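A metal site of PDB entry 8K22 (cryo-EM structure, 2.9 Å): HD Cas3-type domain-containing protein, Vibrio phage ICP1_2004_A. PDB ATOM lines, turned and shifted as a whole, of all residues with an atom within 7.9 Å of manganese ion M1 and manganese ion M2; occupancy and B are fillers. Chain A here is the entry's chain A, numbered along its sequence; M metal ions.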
ATOM      1  N   ALA A 108     -18.355  14.378 -19.208  1.00  0.00           N
ATOM      2  CA  ALA A 108     -19.777  14.585 -19.459  1.00  0.00           C
ATOM      3  C   ALA A 108     -20.008  15.431 -20.712  1.00  0.00           C
ATOM      4  O   ALA A 108     -21.071  15.326 -21.337  1.00  0.00           O
ATOM      5  CB  ALA A 108     -20.431  15.235 -18.248  1.00  0.00           C
ATOM      6  N   HIS A 111     -19.400  12.431 -23.206  1.00  0.00           N
ATOM      7  CA  HIS A 111     -20.019  11.142 -22.945  1.00  0.00           C
ATOM      8  C   HIS A 111     -20.943  10.702 -24.062  1.00  0.00           C
ATOM      9  O   HIS A 111     -21.182   9.493 -24.232  1.00  0.00           O
ATOM     10  CB  HIS A 111     -20.786  11.182 -21.619  1.00  0.00           C
ATOM     11  CG  HIS A 111     -22.197  11.672 -21.739  1.00  0.00           C
ATOM     12  ND1 HIS A 111     -22.508  12.925 -22.207  1.00  0.00           N
ATOM     13  CD2 HIS A 111     -23.380  11.082 -21.440  1.00  0.00           C
ATOM     14  CE1 HIS A 111     -23.815  13.089 -22.217  1.00  0.00           C
ATOM     15  NE2 HIS A 111     -24.371  11.986 -21.742  1.00  0.00           N
ATOM     16  N   ASP A 112     -21.469  11.632 -24.855  1.00  0.00           N
ATOM     17  CA  ASP A 112     -22.415  11.325 -25.909  1.00  0.00           C
ATOM     18  C   ASP A 112     -21.963  11.909 -27.243  1.00  0.00           C
ATOM     19  O   ASP A 112     -22.772  12.376 -28.038  1.00  0.00           O
ATOM     20  CB  ASP A 112     -23.819  11.810 -25.550  1.00  0.00           C
ATOM     21  CG  ASP A 112     -24.577  10.811 -24.707  1.00  0.00           C
ATOM     22  OD1 ASP A 112     -24.088   9.683 -24.516  1.00  0.00           O
ATOM     23  OD2 ASP A 112     -25.684  11.152 -24.230  1.00  0.00           O
ATOM     24  N   LEU A 113     -20.660  11.897 -27.485  1.00  0.00           N
ATOM     25  CA  LEU A 113     -20.154  12.302 -28.793  1.00  0.00           C
ATOM     26  C   LEU A 113     -20.449  11.246 -29.850  1.00  0.00           C
ATOM     27  O   LEU A 113     -20.478  11.558 -31.052  1.00  0.00           O
ATOM     28  CB  LEU A 113     -18.663  12.567 -28.730  1.00  0.00           C
ATOM     29  CG  LEU A 113     -18.165  13.832 -28.030  1.00  0.00           C
ATOM     30  CD1 LEU A 113     -16.656  13.790 -27.952  1.00  0.00           C
ATOM     31  CD2 LEU A 113     -18.628  15.057 -28.783  1.00  0.00           C
ATOM     32  N   LYS A 115     -23.196   9.543 -30.389  1.00  0.00           N
ATOM     33  CA  LYS A 115     -24.530   9.514 -30.970  1.00  0.00           C
ATOM     34  C   LYS A 115     -24.619  10.291 -32.274  1.00  0.00           C
ATOM     35  O   LYS A 115     -25.684  10.287 -32.902  1.00  0.00           O
ATOM     36  CB  LYS A 115     -25.571  10.078 -29.994  1.00  0.00           C
ATOM     37  CG  LYS A 115     -25.828   9.239 -28.772  1.00  0.00           C
ATOM     38  CD  LYS A 115     -26.779   9.936 -27.837  1.00  0.00           C
ATOM     39  CE  LYS A 115     -27.012   9.130 -26.575  1.00  0.00           C
ATOM     40  NZ  LYS A 115     -27.653   9.924 -25.506  1.00  0.00           N
ATOM     41  N   PHE A 120     -27.048   6.145 -35.281  1.00  0.00           N
ATOM     42  CA  PHE A 120     -27.874   6.607 -34.172  1.00  0.00           C
ATOM     43  C   PHE A 120     -28.953   7.571 -34.637  1.00  0.00           C
ATOM     44  O   PHE A 120     -30.040   7.610 -34.047  1.00  0.00           O
ATOM     45  CB  PHE A 120     -27.010   7.270 -33.103  1.00  0.00           C
ATOM     46  CG  PHE A 120     -27.556   7.148 -31.720  1.00  0.00           C
ATOM     47  CD1 PHE A 120     -28.463   8.076 -31.232  1.00  0.00           C
ATOM     48  CD2 PHE A 120     -27.173   6.098 -30.888  1.00  0.00           C
ATOM     49  CE1 PHE A 120     -28.981   7.960 -29.955  1.00  0.00           C
ATOM     50  CE2 PHE A 120     -27.682   5.982 -29.614  1.00  0.00           C
ATOM     51  CZ  PHE A 120     -28.586   6.923 -29.146  1.00  0.00           C
ATOM     52  N   ARG A 135     -21.929   0.447 -29.245  1.00  0.00           N
ATOM     53  CA  ARG A 135     -22.643   1.403 -28.411  1.00  0.00           C
ATOM     54  C   ARG A 135     -21.992   2.778 -28.517  1.00  0.00           C
ATOM     55  O   ARG A 135     -20.781   2.904 -28.714  1.00  0.00           O
ATOM     56  CB  ARG A 135     -22.664   0.932 -26.961  1.00  0.00           C
ATOM     57  CG  ARG A 135     -23.276  -0.447 -26.773  1.00  0.00           C
ATOM     58  CD  ARG A 135     -23.627  -0.700 -25.321  1.00  0.00           C
ATOM     59  NE  ARG A 135     -24.330   0.435 -24.728  1.00  0.00           N
ATOM     60  CZ  ARG A 135     -25.637   0.604 -24.768  1.00  0.00           C
ATOM     61  NH1 ARG A 135     -26.436  -0.281 -25.352  1.00  0.00           N
ATOM     62  NH2 ARG A 135     -26.169   1.685 -24.202  1.00  0.00           N
ATOM     63  N   HIS A 136     -22.831   3.818 -28.377  1.00  0.00           N
ATOM     64  CA  HIS A 136     -22.389   5.185 -28.627  1.00  0.00           C
ATOM     65  C   HIS A 136     -21.378   5.675 -27.596  1.00  0.00           C
ATOM     66  O   HIS A 136     -20.611   6.598 -27.896  1.00  0.00           O
ATOM     67  CB  HIS A 136     -23.595   6.123 -28.633  1.00  0.00           C
ATOM     68  CG  HIS A 136     -24.327   6.175 -27.328  1.00  0.00           C
ATOM     69  ND1 HIS A 136     -25.381   5.346 -27.029  1.00  0.00           N
ATOM     70  CD2 HIS A 136     -24.148   6.969 -26.243  1.00  0.00           C
ATOM     71  CE1 HIS A 136     -25.821   5.612 -25.820  1.00  0.00           C
ATOM     72  NE2 HIS A 136     -25.092   6.593 -25.314  1.00  0.00           N
ATOM     73  N   GLU A 137     -21.359   5.079 -26.396  1.00  0.00           N
ATOM     74  CA  GLU A 137     -20.315   5.395 -25.428  1.00  0.00           C
ATOM     75  C   GLU A 137     -18.946   4.977 -25.946  1.00  0.00           C
ATOM     76  O   GLU A 137     -17.968   5.709 -25.796  1.00  0.00           O
ATOM     77  CB  GLU A 137     -20.616   4.742 -24.084  1.00  0.00           C
ATOM     78  CG  GLU A 137     -21.142   3.330 -24.168  1.00  0.00           C
ATOM     79  CD  GLU A 137     -22.644   3.254 -24.075  1.00  0.00           C
ATOM     80  OE1 GLU A 137     -23.317   4.228 -24.466  1.00  0.00           O
ATOM     81  OE2 GLU A 137     -23.160   2.211 -23.604  1.00  0.00           O
ATOM     82  N   SER A 140     -17.954   7.452 -28.760  1.00  0.00           N
ATOM     83  CA  SER A 140     -17.431   8.682 -28.171  1.00  0.00           C
ATOM     84  C   SER A 140     -16.053   8.472 -27.562  1.00  0.00           C
ATOM     85  O   SER A 140     -15.201   9.363 -27.618  1.00  0.00           O
ATOM     86  CB  SER A 140     -18.407   9.212 -27.127  1.00  0.00           C
ATOM     87  OG  SER A 140     -18.768   8.203 -26.210  1.00  0.00           O
ATOM     88  N   ILE A 183     -16.163   7.900 -19.970  1.00  0.00           N
ATOM     89  CA  ILE A 183     -16.957   8.027 -21.185  1.00  0.00           C
ATOM     90  C   ILE A 183     -17.576   6.687 -21.566  1.00  0.00           C
ATOM     91  O   ILE A 183     -18.772   6.593 -21.841  1.00  0.00           O
ATOM     92  CB  ILE A 183     -16.087   8.591 -22.324  1.00  0.00           C
ATOM     93  CG1 ILE A 183     -15.879  10.094 -22.146  1.00  0.00           C
ATOM     94  CG2 ILE A 183     -16.694   8.327 -23.682  1.00  0.00           C
ATOM     95  CD1 ILE A 183     -14.650  10.571 -22.835  1.00  0.00           C
ATOM     96  N   HIS A 186     -20.403   5.095 -18.924  1.00  0.00           N
ATOM     97  CA  HIS A 186     -21.485   5.943 -18.453  1.00  0.00           C
ATOM     98  C   HIS A 186     -22.847   5.281 -18.608  1.00  0.00           C
ATOM     99  O   HIS A 186     -23.849   5.845 -18.161  1.00  0.00           O
ATOM    100  CB  HIS A 186     -21.441   7.291 -19.179  1.00  0.00           C
ATOM    101  CG  HIS A 186     -22.276   7.354 -20.422  1.00  0.00           C
ATOM    102  ND1 HIS A 186     -21.826   6.886 -21.637  1.00  0.00           N
ATOM    103  CD2 HIS A 186     -23.518   7.840 -20.634  1.00  0.00           C
ATOM    104  CE1 HIS A 186     -22.758   7.072 -22.546  1.00  0.00           C
ATOM    105  NE2 HIS A 186     -23.793   7.659 -21.976  1.00  0.00           N
ATOM    106  N   HIS A 187     -22.909   4.106 -19.241  1.00  0.00           N
ATOM    107  CA  HIS A 187     -24.107   3.284 -19.267  1.00  0.00           C
ATOM    108  C   HIS A 187     -23.882   1.910 -18.650  1.00  0.00           C
ATOM    109  O   HIS A 187     -24.691   1.473 -17.821  1.00  0.00           O
ATOM    110  CB  HIS A 187     -24.629   3.131 -20.710  1.00  0.00           C
ATOM    111  CG  HIS A 187     -25.527   4.253 -21.136  1.00  0.00           C
ATOM    112  ND1 HIS A 187     -25.400   4.877 -22.371  1.00  0.00           N
ATOM    113  CD2 HIS A 187     -26.553   4.861 -20.511  1.00  0.00           C
ATOM    114  CE1 HIS A 187     -26.323   5.808 -22.477  1.00  0.00           C
ATOM    115  NE2 HIS A 187     -27.035   5.827 -21.356  1.00  0.00           N
ATOM    116  N   LEU A 276     -21.787  10.925 -12.868  1.00  0.00           N
ATOM    117  CA  LEU A 276     -22.040  11.049 -14.293  1.00  0.00           C
ATOM    118  C   LEU A 276     -23.348  10.383 -14.692  1.00  0.00           C
ATOM    119  O   LEU A 276     -24.101  10.931 -15.505  1.00  0.00           O
ATOM    120  CB  LEU A 276     -20.859  10.480 -15.082  1.00  0.00           C
ATOM    121  CG  LEU A 276     -20.974  10.401 -16.602  1.00  0.00           C
ATOM    122  CD1 LEU A 276     -21.313  11.754 -17.182  1.00  0.00           C
ATOM    123  CD2 LEU A 276     -19.652   9.922 -17.168  1.00  0.00           C
ATOM    124  N   GLY A 279     -26.163  12.760 -13.383  1.00  0.00           N
ATOM    125  CA  GLY A 279     -26.430  13.866 -14.279  1.00  0.00           C
ATOM    126  C   GLY A 279     -27.054  13.443 -15.594  1.00  0.00           C
ATOM    127  O   GLY A 279     -27.958  14.104 -16.109  1.00  0.00           O
ATOM    128  N   ASP A 280     -26.593  12.314 -16.155  1.00  0.00           N
ATOM    129  CA  ASP A 280     -27.114  11.829 -17.421  1.00  0.00           C
ATOM    130  C   ASP A 280     -28.565  11.402 -17.310  1.00  0.00           C
ATOM    131  O   ASP A 280     -29.398  11.775 -18.146  1.00  0.00           O
ATOM    132  CB  ASP A 280     -26.249  10.675 -17.944  1.00  0.00           C
ATOM    133  CG  ASP A 280     -26.712  10.158 -19.289  1.00  0.00           C
ATOM    134  OD1 ASP A 280     -27.089  10.989 -20.140  1.00  0.00           O
ATOM    135  OD2 ASP A 280     -26.687   8.932 -19.489  1.00  0.00           O
ATOM    136  N   SER A 281     -28.903  10.655 -16.260  1.00  0.00           N
ATOM    137  CA  SER A 281     -30.295  10.234 -16.072  1.00  0.00           C
ATOM    138  C   SER A 281     -31.171  11.402 -15.639  1.00  0.00           C
ATOM    139  O   SER A 281     -32.366  11.419 -15.971  1.00  0.00           O
ATOM    140  CB  SER A 281     -30.353   9.102 -15.047  1.00  0.00           C
ATOM    141  OG  SER A 281     -29.534   9.385 -13.931  1.00  0.00           O
ATOM    142  N   PHE A 283     -30.819  14.550 -16.686  1.00  0.00           N
ATOM    143  CA  PHE A 283     -31.166  15.312 -17.881  1.00  0.00           C
ATOM    144  C   PHE A 283     -31.973  14.484 -18.881  1.00  0.00           C
ATOM    145  O   PHE A 283     -32.737  15.058 -19.663  1.00  0.00           O
ATOM    146  CB  PHE A 283     -29.912  15.867 -18.555  1.00  0.00           C
ATOM    147  CG  PHE A 283     -30.199  17.074 -19.383  1.00  0.00           C
ATOM    148  CD1 PHE A 283     -30.693  18.231 -18.795  1.00  0.00           C
ATOM    149  CD2 PHE A 283     -29.998  17.058 -20.754  1.00  0.00           C
ATOM    150  CE1 PHE A 283     -30.967  19.347 -19.558  1.00  0.00           C
ATOM    151  CE2 PHE A 283     -30.282  18.174 -21.514  1.00  0.00           C
ATOM    152  CZ  PHE A 283     -30.763  19.319 -20.922  1.00  0.00           C
ATOM    153  N   SER A 284     -31.813  13.158 -18.878  1.00  0.00           N
ATOM    154  CA  SER A 284     -32.611  12.321 -19.764  1.00  0.00           C
ATOM    155  C   SER A 284     -34.036  12.127 -19.268  1.00  0.00           C
ATOM    156  O   SER A 284     -34.916  11.788 -20.072  1.00  0.00           O
ATOM    157  CB  SER A 284     -31.937  10.962 -19.956  1.00  0.00           C
ATOM    158  OG  SER A 284     -30.800  11.072 -20.795  1.00  0.00           O
ATOM    159  N   ALA A 297     -30.245  13.314 -29.475  1.00  0.00           N
ATOM    160  CA  ALA A 297     -29.720  12.367 -28.503  1.00  0.00           C
ATOM    161  C   ALA A 297     -30.759  11.375 -28.012  1.00  0.00           C
ATOM    162  O   ALA A 297     -30.547  10.164 -28.103  1.00  0.00           O
ATOM    163  CB  ALA A 297     -29.138  13.123 -27.298  1.00  0.00           C
ATOM    164  N   ASN A 298     -31.871  11.861 -27.486  1.00  0.00           N
ATOM    165  CA  ASN A 298     -32.854  11.013 -26.829  1.00  0.00           C
ATOM    166  C   ASN A 298     -34.210  11.171 -27.498  1.00  0.00           C
ATOM    167  O   ASN A 298     -34.420  12.036 -28.359  1.00  0.00           O
ATOM    168  CB  ASN A 298     -32.953  11.350 -25.340  1.00  0.00           C
ATOM    169  CG  ASN A 298     -31.615  11.741 -24.741  1.00  0.00           C
ATOM    170  OD1 ASN A 298     -31.360  12.912 -24.466  1.00  0.00           O
ATOM    171  ND2 ASN A 298     -30.747  10.759 -24.549  1.00  0.00           N
ATOM    172  N   GLN A 307     -34.224  16.948 -27.434  1.00  0.00           N
ATOM    173  CA  GLN A 307     -32.941  16.990 -26.727  1.00  0.00           C
ATOM    174  C   GLN A 307     -31.764  16.845 -27.699  1.00  0.00           C
ATOM    175  O   GLN A 307     -31.098  15.800 -27.759  1.00  0.00           O
ATOM    176  CB  GLN A 307     -32.873  15.950 -25.611  1.00  0.00           C
ATOM    177  CG  GLN A 307     -33.011  16.529 -24.228  1.00  0.00           C
ATOM    178  CD  GLN A 307     -33.227  15.470 -23.167  1.00  0.00           C
ATOM    179  OE1 GLN A 307     -33.701  14.373 -23.460  1.00  0.00           O
ATOM    180  NE2 GLN A 307     -32.885  15.796 -21.931  1.00  0.00           N
ATOM    181  N   LEU A 309     -28.112  17.302 -29.366  1.00  0.00           N
ATOM    182  CA  LEU A 309     -26.969  16.695 -28.679  1.00  0.00           C
ATOM    183  C   LEU A 309     -26.057  17.738 -28.043  1.00  0.00           C
ATOM    184  O   LEU A 309     -25.399  17.428 -27.039  1.00  0.00           O
ATOM    185  CB  LEU A 309     -26.191  15.820 -29.660  1.00  0.00           C
ATOM    186  CG  LEU A 309     -25.188  14.806 -29.113  1.00  0.00           C
ATOM    187  CD1 LEU A 309     -25.627  14.184 -27.802  1.00  0.00           C
ATOM    188  CD2 LEU A 309     -24.952  13.734 -30.165  1.00  0.00           C
ATOM    189  N   HIS A 312     -27.943  18.635 -25.008  1.00  0.00           N
ATOM    190  CA  HIS A 312     -27.966  17.423 -24.191  1.00  0.00           C
ATOM    191  C   HIS A 312     -26.649  17.225 -23.450  1.00  0.00           C
ATOM    192  O   HIS A 312     -26.647  16.896 -22.263  1.00  0.00           O
ATOM    193  CB  HIS A 312     -28.256  16.194 -25.054  1.00  0.00           C
ATOM    194  CG  HIS A 312     -28.076  14.905 -24.321  1.00  0.00           C
ATOM    195  ND1 HIS A 312     -28.936  14.476 -23.334  1.00  0.00           N
ATOM    196  CD2 HIS A 312     -27.109  13.955 -24.426  1.00  0.00           C
ATOM    197  CE1 HIS A 312     -28.520  13.318 -22.864  1.00  0.00           C
ATOM    198  NE2 HIS A 312     -27.419  12.974 -23.512  1.00  0.00           N
ATOM    199  N   LEU A 313     -25.519  17.415 -24.155  1.00  0.00           N
ATOM    200  CA  LEU A 313     -24.215  17.314 -23.511  1.00  0.00           C
ATOM    201  C   LEU A 313     -24.036  18.386 -22.454  1.00  0.00           C
ATOM    202  O   LEU A 313     -23.516  18.119 -21.361  1.00  0.00           O
ATOM    203  CB  LEU A 313     -23.107  17.417 -24.556  1.00  0.00           C
ATOM    204  CG  LEU A 313     -22.818  16.168 -25.400  1.00  0.00           C
ATOM    205  CD1 LEU A 313     -22.177  16.568 -26.713  1.00  0.00           C
ATOM    206  CD2 LEU A 313     -21.933  15.207 -24.641  1.00  0.00           C
ATOM    207  N   VAL A 316     -26.316  17.425 -19.410  1.00  0.00           N
ATOM    208  CA  VAL A 316     -25.737  16.326 -18.655  1.00  0.00           C
ATOM    209  C   VAL A 316     -24.507  16.795 -17.876  1.00  0.00           C
ATOM    210  O   VAL A 316     -24.323  16.432 -16.715  1.00  0.00           O
ATOM    211  CB  VAL A 316     -25.409  15.142 -19.597  1.00  0.00           C
ATOM    212  CG1 VAL A 316     -24.513  14.114 -18.930  1.00  0.00           C
ATOM    213  CG2 VAL A 316     -26.693  14.482 -20.047  1.00  0.00           C
HETATM  214 MN    MN M   1     -26.549  11.243 -22.238  1.00  0.00          MN
HETATM  215 MN    MN M   2     -25.490   7.923 -23.474  1.00  0.00          MN
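Manganese ion M1 is bound by OD2 of Asp 112 (2.2 Å), OD1 of Asp 280 (2.2 Å), NE2 of His 312 (2.3 Å) and NE2 of His 111 (2.4 Å).
Lys 115 touches manganese ion M2.
His 187 touches manganese ion M2 (CE1 to MN, 2.5 Å).
Of the 26 residues printed, 5 come within 4 Å of manganese ion M2.
The nearest printed residue that does not touch manganese ion M2 is Asp 280 (4.3 Å).
A ring nitrogen (ND1) of His 312 sits at hydrogen-bond distance from the side-chain amide oxygen (OD1) of Asn 298.
O of His 136 sits at hydrogen-bond distance from OG of Ser 140, at 3.0 Å.
ND1 of His 187 sits at hydrogen-bond distance from OE1 of Glu 137.
O of Ala 108 is in hydrogen-bond range of ND1 of His 111 (2.9 Å).
A ring nitrogen (ND1) of His 136 lies close to the side-chain carboxylate of Glu 137.
The backbone carbonyl oxygen (O) of His 111 lies within hydrogen-bond range of the side-chain hydroxyl (OG) of Ser 140.
ND1 of His 186 is in hydrogen-bond range of O of Ile 183.
A ring nitrogen (ND1) of His 187 sits close to a ring nitrogen (NE2) of His 186, at 3.2 Å.
Lys 115 touches manganese ion M1.
Val 316 touches manganese ion M1 (CG2 to MN, 3.9 Å).
Six residues have an atom within 4 Å of manganese ion M1: His 111, Asp 112, Lys 115, Asp 280, His 312 and Val 316.
Along chain A the residues within 4 Å of manganese ion M1 span positions 111 to 316.
Manganese ion M2 is bound by NE2 of His 186 (2.3 Å).
Manganese ion M2 is bound by NE2 of His 136 (2.3 Å).
OD1 of Asp 112 binds manganese ion M2, 2.5 Å away.
Manganese ion M2 has three donor atoms within binding distance.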
